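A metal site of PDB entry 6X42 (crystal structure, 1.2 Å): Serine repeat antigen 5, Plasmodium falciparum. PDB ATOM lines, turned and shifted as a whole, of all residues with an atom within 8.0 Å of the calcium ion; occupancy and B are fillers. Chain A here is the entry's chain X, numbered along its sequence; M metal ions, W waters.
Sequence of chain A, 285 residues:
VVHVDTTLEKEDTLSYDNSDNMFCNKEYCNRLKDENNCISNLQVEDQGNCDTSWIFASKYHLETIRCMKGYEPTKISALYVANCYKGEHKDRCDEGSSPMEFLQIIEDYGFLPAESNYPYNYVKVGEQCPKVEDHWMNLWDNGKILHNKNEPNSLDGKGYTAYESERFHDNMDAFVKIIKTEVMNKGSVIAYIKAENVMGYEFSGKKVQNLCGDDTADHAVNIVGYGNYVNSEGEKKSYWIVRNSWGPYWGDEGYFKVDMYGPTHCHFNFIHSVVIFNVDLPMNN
The nearest printed residue that does not touch the calcium ion is Cys 212 (4.9 Å).
The calcium ion is bound by OE2 of Glu 196 (2.3 Å). The side-chain amide oxygen (OD1) of Asn 197 binds the calcium ion (2.4 Å). Water W1 is bound to the calcium ion (2.4 Å). The calcium ion is bound by OD2 of Asp 214, at 2.4 Å. OD1 of Asp 214 binds the calcium ion (2.6 Å).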
ATOM      1  N   LYS A 194     -26.828  19.341  -5.449  1.00  0.00           N
ATOM      2  CA  LYS A 194     -26.795  20.649  -6.097  1.00  0.00           C
ATOM      3  C   LYS A 194     -25.804  20.558  -7.250  1.00  0.00           C
ATOM      4  O   LYS A 194     -24.631  20.232  -7.048  1.00  0.00           O
ATOM      5  CB  LYS A 194     -26.433  21.766  -5.107  1.00  0.00           C
ATOM      6  CG  LYS A 194     -26.957  23.137  -5.564  1.00  0.00           C
ATOM      7  CD  LYS A 194     -26.820  24.200  -4.504  1.00  0.00           C
ATOM      8  CE  LYS A 194     -27.626  25.442  -4.849  1.00  0.00           C
ATOM      9  NZ  LYS A 194     -27.424  26.488  -3.811  1.00  0.00           N
ATOM     10  N   ALA A 195     -26.288  20.829  -8.469  1.00  0.00           N
ATOM     11  CA  ALA A 195     -25.484  20.613  -9.669  1.00  0.00           C
ATOM     12  C   ALA A 195     -24.169  21.379  -9.601  1.00  0.00           C
ATOM     13  O   ALA A 195     -23.135  20.901 -10.097  1.00  0.00           O
ATOM     14  CB  ALA A 195     -26.251  21.014 -10.928  1.00  0.00           C
ATOM     15  N   GLU A 196     -24.189  22.587  -9.023  1.00  0.00           N
ATOM     16  CA  GLU A 196     -22.959  23.368  -8.948  1.00  0.00           C
ATOM     17  C   GLU A 196     -21.809  22.553  -8.348  1.00  0.00           C
ATOM     18  O   GLU A 196     -20.647  22.753  -8.710  1.00  0.00           O
ATOM     19  CB  GLU A 196     -23.175  24.648  -8.113  1.00  0.00           C
ATOM     20  CG  GLU A 196     -23.257  24.420  -6.609  1.00  0.00           C
ATOM     21  CD  GLU A 196     -23.364  25.694  -5.769  1.00  0.00           C
ATOM     22  OE1 GLU A 196     -23.946  26.690  -6.261  1.00  0.00           O
ATOM     23  OE2 GLU A 196     -22.941  25.653  -4.594  1.00  0.00           O
ATOM     24  N   ASN A 197     -22.135  21.637  -7.432  1.00  0.00           N
ATOM     25  CA  ASN A 197     -21.108  20.974  -6.647  1.00  0.00           C
ATOM     26  C   ASN A 197     -20.272  20.016  -7.475  1.00  0.00           C
ATOM     27  O   ASN A 197     -19.171  19.671  -7.049  1.00  0.00           O
ATOM     28  CB  ASN A 197     -21.720  20.241  -5.462  1.00  0.00           C
ATOM     29  CG  ASN A 197     -22.233  21.211  -4.411  1.00  0.00           C
ATOM     30  OD1 ASN A 197     -21.756  22.338  -4.340  1.00  0.00           O
ATOM     31  ND2 ASN A 197     -23.195  20.794  -3.615  1.00  0.00           N
ATOM     32  N   VAL A 198     -20.757  19.602  -8.652  1.00  0.00           N
ATOM     33  CA  VAL A 198     -19.998  18.703  -9.534  1.00  0.00           C
ATOM     34  C   VAL A 198     -19.431  19.426 -10.746  1.00  0.00           C
ATOM     35  O   VAL A 198     -18.929  18.778 -11.668  1.00  0.00           O
ATOM     36  CB  VAL A 198     -20.811  17.457  -9.941  1.00  0.00           C
ATOM     37  CG1 VAL A 198     -21.334  16.730  -8.717  1.00  0.00           C
ATOM     38  CG2 VAL A 198     -21.971  17.804 -10.868  1.00  0.00           C
ATOM     39  N   LEU A 211     -16.286  16.677  -0.545  1.00  0.00           N
ATOM     40  CA  LEU A 211     -16.784  18.034  -0.448  1.00  0.00           C
ATOM     41  C   LEU A 211     -18.099  18.049   0.321  1.00  0.00           C
ATOM     42  O   LEU A 211     -18.741  17.019   0.504  1.00  0.00           O
ATOM     43  CB  LEU A 211     -16.991  18.638  -1.842  1.00  0.00           C
ATOM     44  CG  LEU A 211     -18.151  18.093  -2.686  1.00  0.00           C
ATOM     45  CD1 LEU A 211     -18.372  19.063  -3.837  1.00  0.00           C
ATOM     46  CD2 LEU A 211     -17.887  16.694  -3.173  1.00  0.00           C
ATOM     47  N   CYS A 212     -18.472  19.244   0.735  1.00  0.00           N
ATOM     48  CA  CYS A 212     -19.747  19.481   1.377  1.00  0.00           C
ATOM     49  C   CYS A 212     -20.857  19.713   0.353  1.00  0.00           C
ATOM     50  O   CYS A 212     -20.623  20.176  -0.760  1.00  0.00           O
ATOM     51  CB  CYS A 212     -19.670  20.771   2.230  1.00  0.00           C
ATOM     52  SG  CYS A 212     -18.354  20.862   3.497  1.00  0.00           S
ATOM     53  N   GLY A 213     -22.073  19.425   0.762  1.00  0.00           N
ATOM     54  CA  GLY A 213     -23.252  19.850   0.052  1.00  0.00           C
ATOM     55  C   GLY A 213     -23.700  21.233   0.471  1.00  0.00           C
ATOM     56  O   GLY A 213     -22.972  21.982   1.154  1.00  0.00           O
ATOM     57  N   ASP A 214     -24.899  21.591   0.050  1.00  0.00           N
ATOM     58  CA  ASP A 214     -25.510  22.873   0.329  1.00  0.00           C
ATOM     59  C   ASP A 214     -26.827  22.636   1.059  1.00  0.00           C
ATOM     60  O   ASP A 214     -27.268  21.506   1.252  1.00  0.00           O
ATOM     61  CB  ASP A 214     -25.736  23.627  -0.987  1.00  0.00           C
ATOM     62  CG  ASP A 214     -24.427  23.944  -1.675  1.00  0.00           C
ATOM     63  OD1 ASP A 214     -23.721  24.906  -1.295  1.00  0.00           O
ATOM     64  OD2 ASP A 214     -24.033  23.215  -2.588  1.00  0.00           O
ATOM     65  N   ASP A 215     -27.492  23.734   1.414  1.00  0.00           N
ATOM     66  CA  ASP A 215     -28.754  23.632   2.133  1.00  0.00           C
ATOM     67  C   ASP A 215     -29.835  22.995   1.268  1.00  0.00           C
ATOM     68  O   ASP A 215     -30.760  22.369   1.794  1.00  0.00           O
ATOM     69  CB  ASP A 215     -29.154  25.049   2.526  1.00  0.00           C
ATOM     70  CG  ASP A 215     -30.173  25.124   3.636  1.00  0.00           C
ATOM     71  OD1 ASP A 215     -30.517  24.104   4.271  1.00  0.00           O
ATOM     72  OD2 ASP A 215     -30.555  26.292   3.904  1.00  0.00           O
ATOM     73  N   THR A 216     -29.727  23.144  -0.054  1.00  0.00           N
ATOM     74  CA  THR A 216     -30.715  22.685  -1.005  1.00  0.00           C
ATOM     75  C   THR A 216     -30.057  21.861  -2.106  1.00  0.00           C
ATOM     76  O   THR A 216     -28.823  21.755  -2.181  1.00  0.00           O
ATOM     77  CB  THR A 216     -31.504  23.850  -1.613  1.00  0.00           C
ATOM     78  OG1 THR A 216     -30.626  24.671  -2.387  1.00  0.00           O
ATOM     79  CG2 THR A 216     -32.162  24.692  -0.541  1.00  0.00           C
ATOM     80  N   PHE A 270     -22.927  16.109   0.908  1.00  0.00           N
ATOM     81  CA  PHE A 270     -23.037  16.213  -0.554  1.00  0.00           C
ATOM     82  C   PHE A 270     -24.336  15.592  -1.089  1.00  0.00           C
ATOM     83  O   PHE A 270     -24.942  16.124  -2.034  1.00  0.00           O
ATOM     84  CB  PHE A 270     -21.801  15.557  -1.196  1.00  0.00           C
ATOM     85  CG  PHE A 270     -21.885  15.479  -2.688  1.00  0.00           C
ATOM     86  CD1 PHE A 270     -21.592  16.566  -3.472  1.00  0.00           C
ATOM     87  CD2 PHE A 270     -22.284  14.315  -3.301  1.00  0.00           C
ATOM     88  CE1 PHE A 270     -21.697  16.480  -4.855  1.00  0.00           C
ATOM     89  CE2 PHE A 270     -22.390  14.219  -4.669  1.00  0.00           C
ATOM     90  CZ  PHE A 270     -22.104  15.311  -5.457  1.00  0.00           C
HETATM   91 CA    CA M   1     -21.898  24.319  -3.028  1.00  0.00          CA
HETATM   92  O   HOH W   1     -20.591  22.888  -1.550  1.00  0.00           O
